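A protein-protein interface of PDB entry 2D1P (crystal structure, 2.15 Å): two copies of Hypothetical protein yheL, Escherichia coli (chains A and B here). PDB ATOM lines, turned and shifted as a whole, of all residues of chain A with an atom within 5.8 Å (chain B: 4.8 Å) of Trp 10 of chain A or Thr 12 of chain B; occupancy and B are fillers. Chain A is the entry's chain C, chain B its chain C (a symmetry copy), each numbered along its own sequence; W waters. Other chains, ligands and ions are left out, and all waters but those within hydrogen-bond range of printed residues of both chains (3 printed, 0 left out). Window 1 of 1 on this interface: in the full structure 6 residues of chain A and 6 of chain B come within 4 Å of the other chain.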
ATOM      1  N   SER A   8     -15.622   5.019  14.797  1.00  0.00           N
ATOM      2  CA  SER A   8     -15.666   3.849  15.655  1.00  0.00           C
ATOM      3  C   SER A   8     -14.286   3.202  15.643  1.00  0.00           C
ATOM      4  O   SER A   8     -13.682   3.048  14.582  1.00  0.00           O
ATOM      5  CB  SER A   8     -16.697   2.862  15.119  1.00  0.00           C
ATOM      6  OG  SER A   8     -16.497   1.579  15.672  1.00  0.00           O
ATOM      7  N   PRO A   9     -13.766   2.820  16.820  1.00  0.00           N
ATOM      8  CA  PRO A   9     -12.444   2.189  16.869  1.00  0.00           C
ATOM      9  C   PRO A   9     -12.367   0.945  15.990  1.00  0.00           C
ATOM     10  O   PRO A   9     -11.295   0.603  15.479  1.00  0.00           O
ATOM     11  CB  PRO A   9     -12.253   1.885  18.356  1.00  0.00           C
ATOM     12  CG  PRO A   9     -13.657   1.816  18.888  1.00  0.00           C
ATOM     13  CD  PRO A   9     -14.345   2.934  18.167  1.00  0.00           C
ATOM     14  N   TRP A  10     -13.511   0.284  15.800  1.00  0.00           N
ATOM     15  CA  TRP A  10     -13.592  -0.917  14.967  1.00  0.00           C
ATOM     16  C   TRP A  10     -13.377  -0.605  13.483  1.00  0.00           C
ATOM     17  O   TRP A  10     -13.048  -1.498  12.700  1.00  0.00           O
ATOM     18  CB  TRP A  10     -14.961  -1.600  15.150  1.00  0.00           C
ATOM     19  CG  TRP A  10     -15.088  -2.375  16.428  1.00  0.00           C
ATOM     20  CD1 TRP A  10     -14.773  -3.694  16.624  1.00  0.00           C
ATOM     21  CD2 TRP A  10     -15.471  -1.862  17.705  1.00  0.00           C
ATOM     22  NE1 TRP A  10     -14.931  -4.027  17.945  1.00  0.00           N
ATOM     23  CE2 TRP A  10     -15.358  -2.921  18.633  1.00  0.00           C
ATOM     24  CE3 TRP A  10     -15.897  -0.605  18.160  1.00  0.00           C
ATOM     25  CZ2 TRP A  10     -15.651  -2.763  19.992  1.00  0.00           C
ATOM     26  CZ3 TRP A  10     -16.192  -0.446  19.516  1.00  0.00           C
ATOM     27  CH2 TRP A  10     -16.064  -1.521  20.416  1.00  0.00           C
ATOM     28  N   LEU A  11     -13.573   0.657  13.096  1.00  0.00           N
ATOM     29  CA  LEU A  11     -13.407   1.070  11.698  1.00  0.00           C
ATOM     30  C   LEU A  11     -12.231   2.038  11.549  1.00  0.00           C
ATOM     31  O   LEU A  11     -12.135   2.781  10.573  1.00  0.00           O
ATOM     32  CB  LEU A  11     -14.688   1.742  11.193  1.00  0.00           C
ATOM     33  CG  LEU A  11     -16.002   0.965  11.366  1.00  0.00           C
ATOM     34  CD1 LEU A  11     -17.161   1.805  10.838  1.00  0.00           C
ATOM     35  CD2 LEU A  11     -15.930  -0.360  10.627  1.00  0.00           C
ATOM     36  N   THR A  12     -11.334   2.013  12.523  1.00  0.00           N
ATOM     37  CA  THR A  12     -10.164   2.884  12.524  1.00  0.00           C
ATOM     38  C   THR A  12      -8.886   2.058  12.546  1.00  0.00           C
ATOM     39  O   THR A  12      -8.860   0.964  13.115  1.00  0.00           O
ATOM     40  CB  THR A  12     -10.179   3.791  13.770  1.00  0.00           C
ATOM     41  OG1 THR A  12     -11.347   4.620  13.733  1.00  0.00           O
ATOM     42  CG2 THR A  12      -8.922   4.662  13.827  1.00  0.00           C
ATOM     43  N   THR A  35     -17.582   5.355  21.505  1.00  0.00           N
ATOM     44  CA  THR A  35     -17.861   3.953  21.795  1.00  0.00           C
ATOM     45  C   THR A  35     -16.634   3.274  22.408  1.00  0.00           C
ATOM     46  O   THR A  35     -16.758   2.262  23.094  1.00  0.00           O
ATOM     47  CB  THR A  35     -18.271   3.175  20.534  1.00  0.00           C
ATOM     48  OG1 THR A  35     -17.322   3.417  19.485  1.00  0.00           O
ATOM     49  CG2 THR A  35     -19.673   3.587  20.092  1.00  0.00           C
ATOM     50  N   ALA A  36     -15.452   3.837  22.171  1.00  0.00           N
ATOM     51  CA  ALA A  36     -14.228   3.261  22.721  1.00  0.00           C
ATOM     52  C   ALA A  36     -14.126   3.537  24.222  1.00  0.00           C
ATOM     53  O   ALA A  36     -13.225   3.035  24.894  1.00  0.00           O
ATOM     54  CB  ALA A  36     -13.006   3.829  22.002  1.00  0.00           C
ATOM     55  N   ASN A  41     -15.250  -2.669  26.667  1.00  0.00           N
ATOM     56  CA  ASN A  41     -15.067  -2.900  25.233  1.00  0.00           C
ATOM     57  C   ASN A  41     -13.613  -3.293  25.001  1.00  0.00           C
ATOM     58  O   ASN A  41     -12.737  -2.908  25.770  1.00  0.00           O
ATOM     59  CB  ASN A  41     -15.438  -1.659  24.406  1.00  0.00           C
ATOM     60  CG  ASN A  41     -14.332  -0.625  24.363  1.00  0.00           C
ATOM     61  OD1 ASN A  41     -14.284   0.288  25.182  1.00  0.00           O
ATOM     62  ND2 ASN A  41     -13.430  -0.775  23.405  1.00  0.00           N
ATOM     63  N   ARG A  42     -13.350  -4.045  23.938  1.00  0.00           N
ATOM     64  CA  ARG A  42     -11.997  -4.511  23.678  1.00  0.00           C
ATOM     65  C   ARG A  42     -10.905  -3.507  23.334  1.00  0.00           C
ATOM     66  O   ARG A  42      -9.738  -3.884  23.269  1.00  0.00           O
ATOM     67  CB  ARG A  42     -12.011  -5.617  22.620  1.00  0.00           C
ATOM     68  CG  ARG A  42     -12.512  -5.214  21.259  1.00  0.00           C
ATOM     69  CD  ARG A  42     -11.582  -5.758  20.185  1.00  0.00           C
ATOM     70  NE  ARG A  42     -12.298  -6.093  18.960  1.00  0.00           N
ATOM     71  CZ  ARG A  42     -11.729  -6.221  17.764  1.00  0.00           C
ATOM     72  NH1 ARG A  42     -10.423  -6.037  17.622  1.00  0.00           N
ATOM     73  NH2 ARG A  42     -12.469  -6.545  16.710  1.00  0.00           N
ATOM     74  N   TYR A  43     -11.253  -2.241  23.119  1.00  0.00           N
ATOM     75  CA  TYR A  43     -10.233  -1.241  22.794  1.00  0.00           C
ATOM     76  C   TYR A  43      -9.824  -0.424  24.010  1.00  0.00           C
ATOM     77  O   TYR A  43      -8.815   0.278  23.990  1.00  0.00           O
ATOM     78  CB  TYR A  43     -10.731  -0.282  21.702  1.00  0.00           C
ATOM     79  CG  TYR A  43     -10.784  -0.905  20.334  1.00  0.00           C
ATOM     80  CD1 TYR A  43     -11.926  -1.578  19.896  1.00  0.00           C
ATOM     81  CD2 TYR A  43      -9.664  -0.891  19.502  1.00  0.00           C
ATOM     82  CE1 TYR A  43     -11.951  -2.228  18.665  1.00  0.00           C
ATOM     83  CE2 TYR A  43      -9.676  -1.543  18.272  1.00  0.00           C
ATOM     84  CZ  TYR A  43     -10.823  -2.213  17.863  1.00  0.00           C
ATOM     85  OH  TYR A  43     -10.822  -2.908  16.676  1.00  0.00           O
ATOM     86  N   LEU B   5     -15.746  -7.044   0.007  1.00  0.00           N
ATOM     87  CA  LEU B   5     -15.061  -6.083   0.869  1.00  0.00           C
ATOM     88  C   LEU B   5     -14.438  -5.002  -0.009  1.00  0.00           C
ATOM     89  O   LEU B   5     -13.478  -5.262  -0.739  1.00  0.00           O
ATOM     90  CB  LEU B   5     -13.967  -6.771   1.692  1.00  0.00           C
ATOM     91  CG  LEU B   5     -13.099  -5.808   2.511  1.00  0.00           C
ATOM     92  CD1 LEU B   5     -13.971  -5.022   3.475  1.00  0.00           C
ATOM     93  CD2 LEU B   5     -12.027  -6.583   3.259  1.00  0.00           C
ATOM     94  N   ARG B   7     -13.537  -1.904   1.335  1.00  0.00           N
ATOM     95  CA  ARG B   7     -12.723  -1.026   2.167  1.00  0.00           C
ATOM     96  C   ARG B   7     -11.443  -1.700   2.636  1.00  0.00           C
ATOM     97  O   ARG B   7     -11.312  -2.923   2.598  1.00  0.00           O
ATOM     98  CB  ARG B   7     -13.514  -0.563   3.390  1.00  0.00           C
ATOM     99  CG  ARG B   7     -14.661   0.383   3.069  1.00  0.00           C
ATOM    100  CD  ARG B   7     -15.443   0.740   4.318  1.00  0.00           C
ATOM    101  NE  ARG B   7     -15.999  -0.452   4.951  1.00  0.00           N
ATOM    102  CZ  ARG B   7     -16.809  -0.429   6.004  1.00  0.00           C
ATOM    103  NH1 ARG B   7     -17.162   0.728   6.550  1.00  0.00           N
ATOM    104  NH2 ARG B   7     -17.279  -1.566   6.503  1.00  0.00           N
ATOM    105  N   SER B   8     -10.500  -0.879   3.076  1.00  0.00           N
ATOM    106  CA  SER B   8      -9.237  -1.377   3.589  1.00  0.00           C
ATOM    107  C   SER B   8      -9.528  -2.219   4.826  1.00  0.00           C
ATOM    108  O   SER B   8     -10.315  -1.814   5.681  1.00  0.00           O
ATOM    109  CB  SER B   8      -8.343  -0.202   3.970  1.00  0.00           C
ATOM    110  OG  SER B   8      -7.297  -0.623   4.819  1.00  0.00           O
ATOM    111  N   PRO B   9      -8.904  -3.402   4.936  1.00  0.00           N
ATOM    112  CA  PRO B   9      -9.143  -4.252   6.106  1.00  0.00           C
ATOM    113  C   PRO B   9      -8.838  -3.530   7.414  1.00  0.00           C
ATOM    114  O   PRO B   9      -9.444  -3.827   8.450  1.00  0.00           O
ATOM    115  CB  PRO B   9      -8.232  -5.456   5.859  1.00  0.00           C
ATOM    116  CG  PRO B   9      -7.171  -4.917   4.940  1.00  0.00           C
ATOM    117  CD  PRO B   9      -7.948  -4.033   4.014  1.00  0.00           C
ATOM    118  N   TRP B  10      -7.914  -2.569   7.357  1.00  0.00           N
ATOM    119  CA  TRP B  10      -7.531  -1.781   8.530  1.00  0.00           C
ATOM    120  C   TRP B  10      -8.656  -0.849   8.990  1.00  0.00           C
ATOM    121  O   TRP B  10      -8.661  -0.398  10.138  1.00  0.00           O
ATOM    122  CB  TRP B  10      -6.273  -0.946   8.223  1.00  0.00           C
ATOM    123  CG  TRP B  10      -5.000  -1.739   8.235  1.00  0.00           C
ATOM    124  CD1 TRP B  10      -4.183  -1.968   9.311  1.00  0.00           C
ATOM    125  CD2 TRP B  10      -4.446  -2.486   7.149  1.00  0.00           C
ATOM    126  NE1 TRP B  10      -3.163  -2.814   8.961  1.00  0.00           N
ATOM    127  CE2 TRP B  10      -3.299  -3.150   7.638  1.00  0.00           C
ATOM    128  CE3 TRP B  10      -4.809  -2.662   5.805  1.00  0.00           C
ATOM    129  CZ2 TRP B  10      -2.513  -3.982   6.834  1.00  0.00           C
ATOM    130  CZ3 TRP B  10      -4.025  -3.491   5.001  1.00  0.00           C
ATOM    131  CH2 TRP B  10      -2.890  -4.143   5.521  1.00  0.00           C
ATOM    132  N   LEU B  11      -9.600  -0.552   8.095  1.00  0.00           N
ATOM    133  CA  LEU B  11     -10.719   0.339   8.420  1.00  0.00           C
ATOM    134  C   LEU B  11     -12.047  -0.421   8.398  1.00  0.00           C
ATOM    135  O   LEU B  11     -13.119   0.172   8.276  1.00  0.00           O
ATOM    136  CB  LEU B  11     -10.777   1.498   7.420  1.00  0.00           C
ATOM    137  CG  LEU B  11      -9.490   2.312   7.215  1.00  0.00           C
ATOM    138  CD1 LEU B  11      -9.734   3.391   6.165  1.00  0.00           C
ATOM    139  CD2 LEU B  11      -9.052   2.941   8.528  1.00  0.00           C
ATOM    140  N   THR B  12     -11.965  -1.736   8.526  1.00  0.00           N
ATOM    141  CA  THR B  12     -13.144  -2.593   8.514  1.00  0.00           C
ATOM    142  C   THR B  12     -13.246  -3.376   9.816  1.00  0.00           C
ATOM    143  O   THR B  12     -12.226  -3.712  10.423  1.00  0.00           O
ATOM    144  CB  THR B  12     -13.058  -3.597   7.348  1.00  0.00           C
ATOM    145  OG1 THR B  12     -13.024  -2.876   6.110  1.00  0.00           O
ATOM    146  CG2 THR B  12     -14.252  -4.554   7.362  1.00  0.00           C
ATOM    147  N   ASP B  13     -14.468  -3.658  10.257  1.00  0.00           N
ATOM    148  CA  ASP B  13     -14.637  -4.440  11.480  1.00  0.00           C
ATOM    149  C   ASP B  13     -14.365  -5.863  11.008  1.00  0.00           C
ATOM    150  O   ASP B  13     -15.291  -6.639  10.783  1.00  0.00           O
ATOM    151  CB  ASP B  13     -16.066  -4.335  12.014  1.00  0.00           C
ATOM    152  CG  ASP B  13     -16.219  -4.974  13.380  1.00  0.00           C
ATOM    153  OD1 ASP B  13     -15.533  -5.984  13.635  1.00  0.00           O
ATOM    154  OD2 ASP B  13     -17.027  -4.479  14.199  1.00  0.00           O
ATOM    155  N   PHE B  14     -13.085  -6.189  10.841  1.00  0.00           N
ATOM    156  CA  PHE B  14     -12.689  -7.496  10.337  1.00  0.00           C
ATOM    157  C   PHE B  14     -13.201  -8.680  11.154  1.00  0.00           C
ATOM    158  O   PHE B  14     -13.600  -9.691  10.587  1.00  0.00           O
ATOM    159  CB  PHE B  14     -11.163  -7.579  10.195  1.00  0.00           C
ATOM    160  CG  PHE B  14     -10.717  -8.341   8.977  1.00  0.00           C
ATOM    161  CD1 PHE B  14     -10.864  -7.793   7.707  1.00  0.00           C
ATOM    162  CD2 PHE B  14     -10.190  -9.623   9.093  1.00  0.00           C
ATOM    163  CE1 PHE B  14     -10.493  -8.508   6.568  1.00  0.00           C
ATOM    164  CE2 PHE B  14      -9.817 -10.344   7.965  1.00  0.00           C
ATOM    165  CZ  PHE B  14      -9.969  -9.784   6.699  1.00  0.00           C
ATOM    166  N   LEU B  17     -16.623  -9.387  10.143  1.00  0.00           N
ATOM    167  CA  LEU B  17     -16.677  -9.986   8.815  1.00  0.00           C
ATOM    168  C   LEU B  17     -16.366 -11.487   8.871  1.00  0.00           C
ATOM    169  O   LEU B  17     -17.061 -12.295   8.253  1.00  0.00           O
ATOM    170  CB  LEU B  17     -15.690  -9.283   7.877  1.00  0.00           C
ATOM    171  CG  LEU B  17     -15.567  -9.809   6.442  1.00  0.00           C
ATOM    172  CD1 LEU B  17     -14.928  -8.735   5.558  1.00  0.00           C
ATOM    173  CD2 LEU B  17     -14.734 -11.075   6.417  1.00  0.00           C
HETATM  174  O   HOH W   1     -12.852  -6.146  14.107  1.00  0.00           O
HETATM  175  O   HOH W   2      -7.365  -1.809  12.380  1.00  0.00           O
HETATM  176  O   HOH W   3     -11.564  -3.888  13.585  1.00  0.00           O
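The backbone carbonyl oxygen of Thr 12 of chain B sits close to the backbone carbonyl oxygen of Trp 10 of chain A, at 3.3 Å.
The backbone carbonyl oxygen of Thr 12 of chain A lies close to the backbone carbonyl oxygen of Trp 10 of chain B (3.3 Å).
Trp 10 of chain A touches Thr 12 of chain B, and with the chains exchanged Thr 12 of chain A touches Trp 10 of chain B.
Leu 11 of chain B touches its own counterpart, Leu 11 of chain A.
5 positions are printed for both chains.
Trp 10 of chain A touches just these residues of chain B: Thr 12 (3.3 Å) and Asp 13 (3.4 Å).
Of the printed residues of chain B, Leu 11 of chain A touches Leu 11 and Asp 13.
Of the printed residues of chain B, Thr 12 of chain A touches Trp 10 (3.3 Å).
Asn 41 of chain A touches none of the printed residues of chain B.
Of the printed residues of chain A, Leu 11 of chain B touches Leu 11 (3.5 Å).
Of chain A, only Trp 10 comes within 4 Å of Thr 12 of chain B.
The nearest residue of chain B that does not touch Trp 10 of chain A is Leu 11 of chain B (4.5 Å).
Water W1 lies within hydrogen-bond range of NH2 of Arg 42 of chain A (2.7 Å), OD1 of Asp 13 of chain B (2.7 Å) and N of Phe 14 of chain B (3.3 Å).
Water W2 bridges the backbone carbonyl oxygen (O) of Trp 10 of chain B (2.9 Å) and the backbone carbonyl oxygen (O) of Thr 12 of chain A (3.2 Å).
Water W3 lies within hydrogen-bond range of O of Trp 10 of chain A (2.9 Å), O of Thr 12 of chain B (3.2 Å) and OH of Tyr 43 of chain A (3.3 Å).
Of the 10 printed residues of chain B, 4 touch a printed residue of chain A.
Hydrophobic or aromatic side chains of chain B that line the printed part of chain A: Leu 11.
Printed residues of chain A that touch a printed residue of chain B: Trp 10, Leu 11 and Thr 12.
Hydrophobic or aromatic side chains of chain A that line the printed part of chain B: Trp 10 and Leu 11.
Among the printed residues, 5 pairs touch across the chains.
Among the printed residues, pairs that only touch across the chains: Trp 10 of chain A with Asp 13 of chain B, Leu 11 of chain A with Leu 11 of chain B and Leu 11 of chain A with Asp 13 of chain B.
OG of Ser 8 of chain A sits close to N of Trp 10 of chain A (3.3 Å).
The backbone carbonyl oxygen of Ser 8 of chain A sits at hydrogen-bond distance from the side-chain hydroxyl of Thr 12 of chain A (2.9 Å).
The side-chain hydroxyl (OG) of Ser 8 of chain B lies close to the backbone NH (N) of Trp 10 of chain B.
The side-chain hydroxyl of Thr 12 of chain B is in hydrogen-bond range of the backbone carbonyl oxygen of Ser 8 of chain B.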
